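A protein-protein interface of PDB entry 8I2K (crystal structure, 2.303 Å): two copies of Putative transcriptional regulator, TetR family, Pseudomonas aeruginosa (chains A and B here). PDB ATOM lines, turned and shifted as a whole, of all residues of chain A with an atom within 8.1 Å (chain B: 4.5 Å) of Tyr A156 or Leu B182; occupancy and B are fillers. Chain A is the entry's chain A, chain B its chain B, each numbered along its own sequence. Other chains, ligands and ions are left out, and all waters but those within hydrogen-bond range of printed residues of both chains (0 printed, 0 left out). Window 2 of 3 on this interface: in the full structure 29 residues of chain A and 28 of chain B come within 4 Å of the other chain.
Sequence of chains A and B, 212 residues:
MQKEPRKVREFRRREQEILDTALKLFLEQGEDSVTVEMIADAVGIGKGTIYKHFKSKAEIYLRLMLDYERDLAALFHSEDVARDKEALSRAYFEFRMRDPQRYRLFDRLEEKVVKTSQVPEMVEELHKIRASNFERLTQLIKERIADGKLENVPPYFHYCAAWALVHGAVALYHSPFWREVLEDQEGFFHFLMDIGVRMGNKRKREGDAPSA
No position is printed for both chains.
The backbone carbonyl oxygen (O) of Tyr A156 lies within hydrogen-bond range of the side-chain sulfur (SG) of Cys A160.
The side-chain hydroxyl of Thr A138 sits close to the backbone carbonyl oxygen of Phe A134 (3.4 Å).
The backbone NH (N) of Phe B177 lies close to the side-chain carboxylate (OE1) of Glu B180, 3.2 Å away.
CE1 of Phe A134 touches CE1 of Phe B177, 3.9 Å away.
Phe B177 touches Tyr A156 (CZ to CD1, 3.8 Å).
Val B181 touches Tyr A156 (CG1 to CE1, 3.3 Å).
Leu B182 touches Tyr A156 (CD1 to CB, 3.5 Å).
Asp B184 touches Phe A157.
CZ of Phe A157 touches N of Phe B188, 3.4 Å away.
SG of Cys A160 touches CE2 of Phe B177 (3.5 Å).
Leu B182 touches Cys A160 (CD2 to SG, 3.8 Å).
Phe B188 touches Cys A160 (CE1 to CB, 3.7 Å).
Printed residues of chain B that touch a printed residue of chain A: Phe B177, Val B181, Leu B182, Asp B184 and Phe B188.
Hydrophobic or aromatic side chains of chain B that line the printed part of chain A: Phe B177, Val B181, Leu B182 and Phe B188.
Of the 17 printed residues of chain A, 4 touch a printed residue of chain B.
Among the printed residues, no Asp or Glu carboxylate lies within 4 Å of a Lys or Arg side-chain nitrogen of the other chain.
Printed residues of chain B within 4 Å of Phe A134: Phe B177.
Lys A142 touches none of the printed residues of chain B.
Ala A162 touches none of the printed residues of chain B.
Printed residues of chain A within 4 Å of Phe B177: Phe A134 (3.9 Å), Tyr A156 (3.8 Å) and Cys A160 (3.5 Å).
Of the printed residues of chain A, Val B181 touches Tyr A156.
Of the printed residues of chain A, Asp B184 touches Phe A157.
Of the printed residues of chain A, Phe B188 touches Phe A157 and Cys A160.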
ATOM      1  N   PHE A 134     -23.104 -21.102 -18.884  1.00  0.00           N
ATOM      2  CA  PHE A 134     -22.415 -22.200 -18.240  1.00  0.00           C
ATOM      3  C   PHE A 134     -21.743 -23.081 -19.269  1.00  0.00           C
ATOM      4  O   PHE A 134     -20.567 -23.442 -19.114  1.00  0.00           O
ATOM      5  CB  PHE A 134     -23.403 -22.993 -17.392  1.00  0.00           C
ATOM      6  CG  PHE A 134     -22.823 -24.157 -16.769  1.00  0.00           C
ATOM      7  CD1 PHE A 134     -21.905 -24.024 -15.759  1.00  0.00           C
ATOM      8  CD2 PHE A 134     -23.201 -25.398 -17.167  1.00  0.00           C
ATOM      9  CE1 PHE A 134     -21.365 -25.143 -15.146  1.00  0.00           C
ATOM     10  CE2 PHE A 134     -22.621 -26.535 -16.581  1.00  0.00           C
ATOM     11  CZ  PHE A 134     -21.715 -26.395 -15.564  1.00  0.00           C
ATOM     12  N   GLU A 135     -22.465 -23.433 -20.337  1.00  0.00           N
ATOM     13  CA  GLU A 135     -21.844 -24.239 -21.380  1.00  0.00           C
ATOM     14  C   GLU A 135     -20.725 -23.470 -22.077  1.00  0.00           C
ATOM     15  O   GLU A 135     -19.734 -24.070 -22.494  1.00  0.00           O
ATOM     16  CB  GLU A 135     -22.861 -24.737 -22.426  1.00  0.00           C
ATOM     17  N   THR A 138     -17.630 -23.492 -19.723  1.00  0.00           N
ATOM     18  CA  THR A 138     -16.936 -24.765 -19.592  1.00  0.00           C
ATOM     19  C   THR A 138     -16.318 -25.195 -20.909  1.00  0.00           C
ATOM     20  O   THR A 138     -15.321 -25.920 -20.901  1.00  0.00           O
ATOM     21  CB  THR A 138     -17.853 -25.846 -19.005  1.00  0.00           C
ATOM     22  OG1 THR A 138     -18.808 -26.290 -19.941  1.00  0.00           O
ATOM     23  CG2 THR A 138     -18.574 -25.283 -17.831  1.00  0.00           C
ATOM     24  N   ILE A 141     -12.945 -23.576 -20.800  1.00  0.00           N
ATOM     25  CA  ILE A 141     -12.148 -24.450 -19.943  1.00  0.00           C
ATOM     26  C   ILE A 141     -11.665 -25.682 -20.706  1.00  0.00           C
ATOM     27  O   ILE A 141     -10.473 -26.013 -20.681  1.00  0.00           O
ATOM     28  CB  ILE A 141     -12.987 -24.853 -18.712  1.00  0.00           C
ATOM     29  CG1 ILE A 141     -13.135 -23.666 -17.762  1.00  0.00           C
ATOM     30  CG2 ILE A 141     -12.403 -26.025 -17.945  1.00  0.00           C
ATOM     31  CD1 ILE A 141     -14.233 -23.842 -16.760  1.00  0.00           C
ATOM     32  N   LYS A 142     -12.592 -26.420 -21.360  1.00  0.00           N
ATOM     33  CA  LYS A 142     -12.168 -27.644 -22.070  1.00  0.00           C
ATOM     34  C   LYS A 142     -11.139 -27.336 -23.162  1.00  0.00           C
ATOM     35  O   LYS A 142     -10.216 -28.124 -23.408  1.00  0.00           O
ATOM     36  CB  LYS A 142     -13.358 -28.380 -22.695  1.00  0.00           C
ATOM     37  CG  LYS A 142     -14.377 -28.910 -21.684  1.00  0.00           C
ATOM     38  CD  LYS A 142     -15.693 -29.205 -22.350  1.00  0.00           C
ATOM     39  CE  LYS A 142     -16.632 -30.030 -21.498  1.00  0.00           C
ATOM     40  NZ  LYS A 142     -18.029 -29.973 -22.125  1.00  0.00           N
ATOM     41  N   ILE A 145      -7.814 -26.772 -21.532  1.00  0.00           N
ATOM     42  CA  ILE A 145      -7.267 -28.079 -21.181  1.00  0.00           C
ATOM     43  C   ILE A 145      -6.687 -28.748 -22.420  1.00  0.00           C
ATOM     44  O   ILE A 145      -5.557 -29.236 -22.416  1.00  0.00           O
ATOM     45  CB  ILE A 145      -8.366 -28.948 -20.546  1.00  0.00           C
ATOM     46  CG1 ILE A 145      -8.775 -28.435 -19.154  1.00  0.00           C
ATOM     47  CG2 ILE A 145      -7.968 -30.385 -20.405  1.00  0.00           C
ATOM     48  CD1 ILE A 145     -10.004 -29.213 -18.558  1.00  0.00           C
ATOM     49  N   VAL A 153      -8.235 -32.137 -15.425  1.00  0.00           N
ATOM     50  CA  VAL A 153      -9.132 -32.603 -14.367  1.00  0.00           C
ATOM     51  C   VAL A 153     -10.523 -32.334 -14.902  1.00  0.00           C
ATOM     52  O   VAL A 153     -10.641 -31.672 -15.938  1.00  0.00           O
ATOM     53  CB  VAL A 153      -8.864 -31.863 -13.055  1.00  0.00           C
ATOM     54  CG1 VAL A 153      -7.439 -32.183 -12.604  1.00  0.00           C
ATOM     55  CG2 VAL A 153      -9.054 -30.419 -13.292  1.00  0.00           C
ATOM     56  N   PRO A 154     -11.587 -32.805 -14.259  1.00  0.00           N
ATOM     57  CA  PRO A 154     -12.938 -32.507 -14.754  1.00  0.00           C
ATOM     58  C   PRO A 154     -13.125 -31.010 -14.925  1.00  0.00           C
ATOM     59  O   PRO A 154     -12.718 -30.205 -14.059  1.00  0.00           O
ATOM     60  CB  PRO A 154     -13.854 -33.089 -13.662  1.00  0.00           C
ATOM     61  CG  PRO A 154     -13.026 -34.208 -13.050  1.00  0.00           C
ATOM     62  CD  PRO A 154     -11.604 -33.650 -13.050  1.00  0.00           C
ATOM     63  N   PRO A 155     -13.725 -30.589 -16.036  1.00  0.00           N
ATOM     64  CA  PRO A 155     -13.885 -29.155 -16.267  1.00  0.00           C
ATOM     65  C   PRO A 155     -14.629 -28.435 -15.161  1.00  0.00           C
ATOM     66  O   PRO A 155     -14.379 -27.236 -14.965  1.00  0.00           O
ATOM     67  CB  PRO A 155     -14.665 -29.100 -17.594  1.00  0.00           C
ATOM     68  CG  PRO A 155     -14.313 -30.365 -18.286  1.00  0.00           C
ATOM     69  CD  PRO A 155     -14.282 -31.376 -17.157  1.00  0.00           C
ATOM     70  N   TYR A 156     -15.524 -29.115 -14.433  1.00  0.00           N
ATOM     71  CA  TYR A 156     -16.236 -28.430 -13.366  1.00  0.00           C
ATOM     72  C   TYR A 156     -15.290 -28.070 -12.216  1.00  0.00           C
ATOM     73  O   TYR A 156     -15.617 -27.182 -11.417  1.00  0.00           O
ATOM     74  CB  TYR A 156     -17.409 -29.294 -12.845  1.00  0.00           C
ATOM     75  CG  TYR A 156     -18.565 -29.577 -13.808  1.00  0.00           C
ATOM     76  CD1 TYR A 156     -19.742 -30.202 -13.351  1.00  0.00           C
ATOM     77  CD2 TYR A 156     -18.478 -29.283 -15.181  1.00  0.00           C
ATOM     78  CE1 TYR A 156     -20.812 -30.486 -14.220  1.00  0.00           C
ATOM     79  CE2 TYR A 156     -19.535 -29.590 -16.074  1.00  0.00           C
ATOM     80  CZ  TYR A 156     -20.706 -30.155 -15.582  1.00  0.00           C
ATOM     81  OH  TYR A 156     -21.754 -30.440 -16.466  1.00  0.00           O
ATOM     82  N   PHE A 157     -14.134 -28.741 -12.094  1.00  0.00           N
ATOM     83  CA  PHE A 157     -13.143 -28.323 -11.089  1.00  0.00           C
ATOM     84  C   PHE A 157     -12.685 -26.884 -11.341  1.00  0.00           C
ATOM     85  O   PHE A 157     -12.568 -26.077 -10.412  1.00  0.00           O
ATOM     86  CB  PHE A 157     -11.899 -29.225 -11.108  1.00  0.00           C
ATOM     87  CG  PHE A 157     -12.057 -30.568 -10.425  1.00  0.00           C
ATOM     88  CD1 PHE A 157     -13.286 -31.163 -10.275  1.00  0.00           C
ATOM     89  CD2 PHE A 157     -10.943 -31.236  -9.956  1.00  0.00           C
ATOM     90  CE1 PHE A 157     -13.398 -32.363  -9.649  1.00  0.00           C
ATOM     91  CE2 PHE A 157     -11.059 -32.474  -9.363  1.00  0.00           C
ATOM     92  CZ  PHE A 157     -12.276 -33.026  -9.206  1.00  0.00           C
ATOM     93  N   HIS A 158     -12.394 -26.559 -12.602  1.00  0.00           N
ATOM     94  CA  HIS A 158     -11.959 -25.215 -12.923  1.00  0.00           C
ATOM     95  C   HIS A 158     -13.123 -24.260 -12.806  1.00  0.00           C
ATOM     96  O   HIS A 158     -12.959 -23.108 -12.396  1.00  0.00           O
ATOM     97  CB  HIS A 158     -11.384 -25.143 -14.343  1.00  0.00           C
ATOM     98  CG  HIS A 158     -10.199 -26.010 -14.568  1.00  0.00           C
ATOM     99  ND1 HIS A 158      -8.928 -25.622 -14.232  1.00  0.00           N
ATOM    100  CD2 HIS A 158     -10.085 -27.215 -15.174  1.00  0.00           C
ATOM    101  CE1 HIS A 158      -8.078 -26.560 -14.615  1.00  0.00           C
ATOM    102  NE2 HIS A 158      -8.762 -27.549 -15.155  1.00  0.00           N
ATOM    103  N   TYR A 159     -14.309 -24.699 -13.214  1.00  0.00           N
ATOM    104  CA  TYR A 159     -15.468 -23.832 -13.090  1.00  0.00           C
ATOM    105  C   TYR A 159     -15.669 -23.420 -11.624  1.00  0.00           C
ATOM    106  O   TYR A 159     -15.936 -22.258 -11.332  1.00  0.00           O
ATOM    107  CB  TYR A 159     -16.699 -24.541 -13.660  1.00  0.00           C
ATOM    108  CG  TYR A 159     -17.958 -23.755 -13.452  1.00  0.00           C
ATOM    109  CD1 TYR A 159     -18.326 -22.743 -14.337  1.00  0.00           C
ATOM    110  CD2 TYR A 159     -18.721 -23.935 -12.344  1.00  0.00           C
ATOM    111  CE1 TYR A 159     -19.454 -21.979 -14.124  1.00  0.00           C
ATOM    112  CE2 TYR A 159     -19.883 -23.161 -12.125  1.00  0.00           C
ATOM    113  CZ  TYR A 159     -20.235 -22.221 -13.033  1.00  0.00           C
ATOM    114  OH  TYR A 159     -21.342 -21.471 -12.867  1.00  0.00           O
ATOM    115  N   CYS A 160     -15.530 -24.370 -10.697  1.00  0.00           N
ATOM    116  CA  CYS A 160     -15.791 -24.102  -9.288  1.00  0.00           C
ATOM    117  C   CYS A 160     -14.677 -23.243  -8.676  1.00  0.00           C
ATOM    118  O   CYS A 160     -14.947 -22.343  -7.882  1.00  0.00           O
ATOM    119  CB  CYS A 160     -15.960 -25.431  -8.542  1.00  0.00           C
ATOM    120  SG  CYS A 160     -17.443 -26.433  -8.738  1.00  0.00           S
ATOM    121  N   ALA A 161     -13.433 -23.514  -9.045  1.00  0.00           N
ATOM    122  CA  ALA A 161     -12.320 -22.648  -8.681  1.00  0.00           C
ATOM    123  C   ALA A 161     -12.583 -21.206  -9.080  1.00  0.00           C
ATOM    124  O   ALA A 161     -12.399 -20.274  -8.278  1.00  0.00           O
ATOM    125  CB  ALA A 161     -11.020 -23.125  -9.339  1.00  0.00           C
ATOM    126  N   ALA A 162     -12.966 -20.998 -10.340  1.00  0.00           N
ATOM    127  CA  ALA A 162     -13.223 -19.646 -10.822  1.00  0.00           C
ATOM    128  C   ALA A 162     -14.312 -18.975 -10.007  1.00  0.00           C
ATOM    129  O   ALA A 162     -14.184 -17.806  -9.619  1.00  0.00           O
ATOM    130  CB  ALA A 162     -13.631 -19.654 -12.293  1.00  0.00           C
ATOM    131  N   TRP A 163     -15.416 -19.692  -9.793  1.00  0.00           N
ATOM    132  CA  TRP A 163     -16.513 -19.182  -8.983  1.00  0.00           C
ATOM    133  C   TRP A 163     -16.022 -18.792  -7.591  1.00  0.00           C
ATOM    134  O   TRP A 163     -16.338 -17.709  -7.085  1.00  0.00           O
ATOM    135  CB  TRP A 163     -17.600 -20.249  -8.886  1.00  0.00           C
ATOM    136  CG  TRP A 163     -18.842 -19.763  -8.298  1.00  0.00           C
ATOM    137  CD1 TRP A 163     -19.948 -19.372  -8.978  1.00  0.00           C
ATOM    138  CD2 TRP A 163     -19.147 -19.613  -6.901  1.00  0.00           C
ATOM    139  NE1 TRP A 163     -20.913 -18.944  -8.106  1.00  0.00           N
ATOM    140  CE2 TRP A 163     -20.460 -19.107  -6.822  1.00  0.00           C
ATOM    141  CE3 TRP A 163     -18.453 -19.868  -5.722  1.00  0.00           C
ATOM    142  CZ2 TRP A 163     -21.093 -18.846  -5.601  1.00  0.00           C
ATOM    143  CZ3 TRP A 163     -19.061 -19.584  -4.513  1.00  0.00           C
ATOM    144  CH2 TRP A 163     -20.371 -19.075  -4.458  1.00  0.00           C
ATOM    145  N   PHE B 177     -24.968 -25.684  -6.445  1.00  0.00           N
ATOM    146  CA  PHE B 177     -23.992 -26.389  -7.315  1.00  0.00           C
ATOM    147  C   PHE B 177     -23.295 -27.501  -6.528  1.00  0.00           C
ATOM    148  O   PHE B 177     -23.727 -28.657  -6.563  1.00  0.00           O
ATOM    149  CB  PHE B 177     -22.924 -25.429  -7.946  1.00  0.00           C
ATOM    150  CG  PHE B 177     -22.213 -26.027  -9.181  1.00  0.00           C
ATOM    151  CD1 PHE B 177     -22.741 -25.880 -10.441  1.00  0.00           C
ATOM    152  CD2 PHE B 177     -21.070 -26.828  -9.036  1.00  0.00           C
ATOM    153  CE1 PHE B 177     -22.135 -26.465 -11.548  1.00  0.00           C
ATOM    154  CE2 PHE B 177     -20.453 -27.414 -10.126  1.00  0.00           C
ATOM    155  CZ  PHE B 177     -20.975 -27.222 -11.392  1.00  0.00           C
ATOM    156  N   TRP B 178     -22.299 -27.153  -5.715  1.00  0.00           N
ATOM    157  CA  TRP B 178     -21.377 -28.150  -5.159  1.00  0.00           C
ATOM    158  C   TRP B 178     -21.936 -29.476  -4.708  1.00  0.00           C
ATOM    159  O   TRP B 178     -21.358 -30.539  -5.000  1.00  0.00           O
ATOM    160  CB  TRP B 178     -20.704 -27.567  -3.958  1.00  0.00           C
ATOM    161  CG  TRP B 178     -19.796 -28.447  -3.233  1.00  0.00           C
ATOM    162  CD1 TRP B 178     -18.491 -28.769  -3.579  1.00  0.00           C
ATOM    163  CD2 TRP B 178     -20.073 -29.141  -2.010  1.00  0.00           C
ATOM    164  NE1 TRP B 178     -17.966 -29.607  -2.619  1.00  0.00           N
ATOM    165  CE2 TRP B 178     -18.874 -29.737  -1.590  1.00  0.00           C
ATOM    166  CE3 TRP B 178     -21.188 -29.236  -1.171  1.00  0.00           C
ATOM    167  CZ2 TRP B 178     -18.794 -30.498  -0.391  1.00  0.00           C
ATOM    168  CZ3 TRP B 178     -21.092 -30.032   0.000  1.00  0.00           C
ATOM    169  CH2 TRP B 178     -19.936 -30.712   0.310  1.00  0.00           C
ATOM    170  N   GLU B 180     -24.693 -31.027  -5.471  1.00  0.00           N
ATOM    171  CA  GLU B 180     -25.631 -31.766  -6.331  1.00  0.00           C
ATOM    172  C   GLU B 180     -25.150 -32.037  -7.747  1.00  0.00           C
ATOM    173  O   GLU B 180     -25.706 -32.967  -8.386  1.00  0.00           O
ATOM    174  CB  GLU B 180     -26.999 -31.047  -6.336  1.00  0.00           C
ATOM    175  CG  GLU B 180     -27.441 -30.216  -7.522  1.00  0.00           C
ATOM    176  CD  GLU B 180     -26.511 -29.105  -7.924  1.00  0.00           C
ATOM    177  OE1 GLU B 180     -25.900 -28.735  -7.023  1.00  0.00           O
ATOM    178  OE2 GLU B 180     -26.196 -28.646  -9.035  1.00  0.00           O
ATOM    179  N   VAL B 181     -24.183 -31.263  -8.278  1.00  0.00           N
ATOM    180  CA  VAL B 181     -23.662 -31.531  -9.615  1.00  0.00           C
ATOM    181  C   VAL B 181     -22.173 -31.878  -9.589  1.00  0.00           C
ATOM    182  O   VAL B 181     -21.706 -32.649 -10.454  1.00  0.00           O
ATOM    183  CB  VAL B 181     -23.948 -30.345 -10.574  1.00  0.00           C
ATOM    184  CG1 VAL B 181     -23.118 -30.438 -11.850  1.00  0.00           C
ATOM    185  CG2 VAL B 181     -25.431 -30.299 -10.915  1.00  0.00           C
ATOM    186  N   LEU B 182     -21.412 -31.328  -8.624  1.00  0.00           N
ATOM    187  CA  LEU B 182     -19.980 -31.626  -8.579  1.00  0.00           C
ATOM    188  C   LEU B 182     -19.769 -33.024  -8.006  1.00  0.00           C
ATOM    189  O   LEU B 182     -20.155 -33.307  -6.860  1.00  0.00           O
ATOM    190  CB  LEU B 182     -19.179 -30.615  -7.774  1.00  0.00           C
ATOM    191  CG  LEU B 182     -17.660 -30.728  -8.082  1.00  0.00           C
ATOM    192  CD1 LEU B 182     -17.250 -30.443  -9.554  1.00  0.00           C
ATOM    193  CD2 LEU B 182     -16.916 -29.835  -7.037  1.00  0.00           C
ATOM    194  N   GLU B 183     -19.111 -33.874  -8.801  1.00  0.00           N
ATOM    195  CA  GLU B 183     -19.041 -35.319  -8.583  1.00  0.00           C
ATOM    196  C   GLU B 183     -17.908 -35.720  -7.628  1.00  0.00           C
ATOM    197  O   GLU B 183     -18.156 -36.328  -6.581  1.00  0.00           O
ATOM    198  CB  GLU B 183     -18.874 -36.028  -9.942  1.00  0.00           C
ATOM    199  CG  GLU B 183     -20.143 -36.556 -10.572  1.00  0.00           C
ATOM    200  CD  GLU B 183     -20.582 -37.899  -9.983  1.00  0.00           C
ATOM    201  OE1 GLU B 183     -20.151 -38.226  -8.852  1.00  0.00           O
ATOM    202  OE2 GLU B 183     -21.377 -38.615 -10.645  1.00  0.00           O
ATOM    203  N   ASP B 184     -16.666 -35.380  -7.970  1.00  0.00           N
ATOM    204  CA  ASP B 184     -15.489 -35.894  -7.265  1.00  0.00           C
ATOM    205  C   ASP B 184     -15.047 -34.852  -6.250  1.00  0.00           C
ATOM    206  O   ASP B 184     -14.133 -34.055  -6.496  1.00  0.00           O
ATOM    207  CB  ASP B 184     -14.384 -36.226  -8.258  1.00  0.00           C
ATOM    208  CG  ASP B 184     -13.099 -36.661  -7.600  1.00  0.00           C
ATOM    209  OD1 ASP B 184     -13.032 -36.743  -6.340  1.00  0.00           O
ATOM    210  OD2 ASP B 184     -12.133 -36.919  -8.366  1.00  0.00           O
ATOM    211  N   PHE B 188     -11.515 -32.659  -5.894  1.00  0.00           N
ATOM    212  CA  PHE B 188     -11.644 -31.217  -6.015  1.00  0.00           C
ATOM    213  C   PHE B 188     -10.925 -30.534  -4.866  1.00  0.00           C
ATOM    214  O   PHE B 188     -10.292 -29.491  -5.046  1.00  0.00           O
ATOM    215  CB  PHE B 188     -13.113 -30.773  -6.030  1.00  0.00           C
ATOM    216  CG  PHE B 188     -13.260 -29.284  -6.043  1.00  0.00           C
ATOM    217  CD1 PHE B 188     -12.879 -28.558  -7.168  1.00  0.00           C
ATOM    218  CD2 PHE B 188     -13.662 -28.605  -4.897  1.00  0.00           C
ATOM    219  CE1 PHE B 188     -12.949 -27.168  -7.180  1.00  0.00           C
ATOM    220  CE2 PHE B 188     -13.730 -27.228  -4.874  1.00  0.00           C
ATOM    221  CZ  PHE B 188     -13.371 -26.485  -6.026  1.00  0.00           C
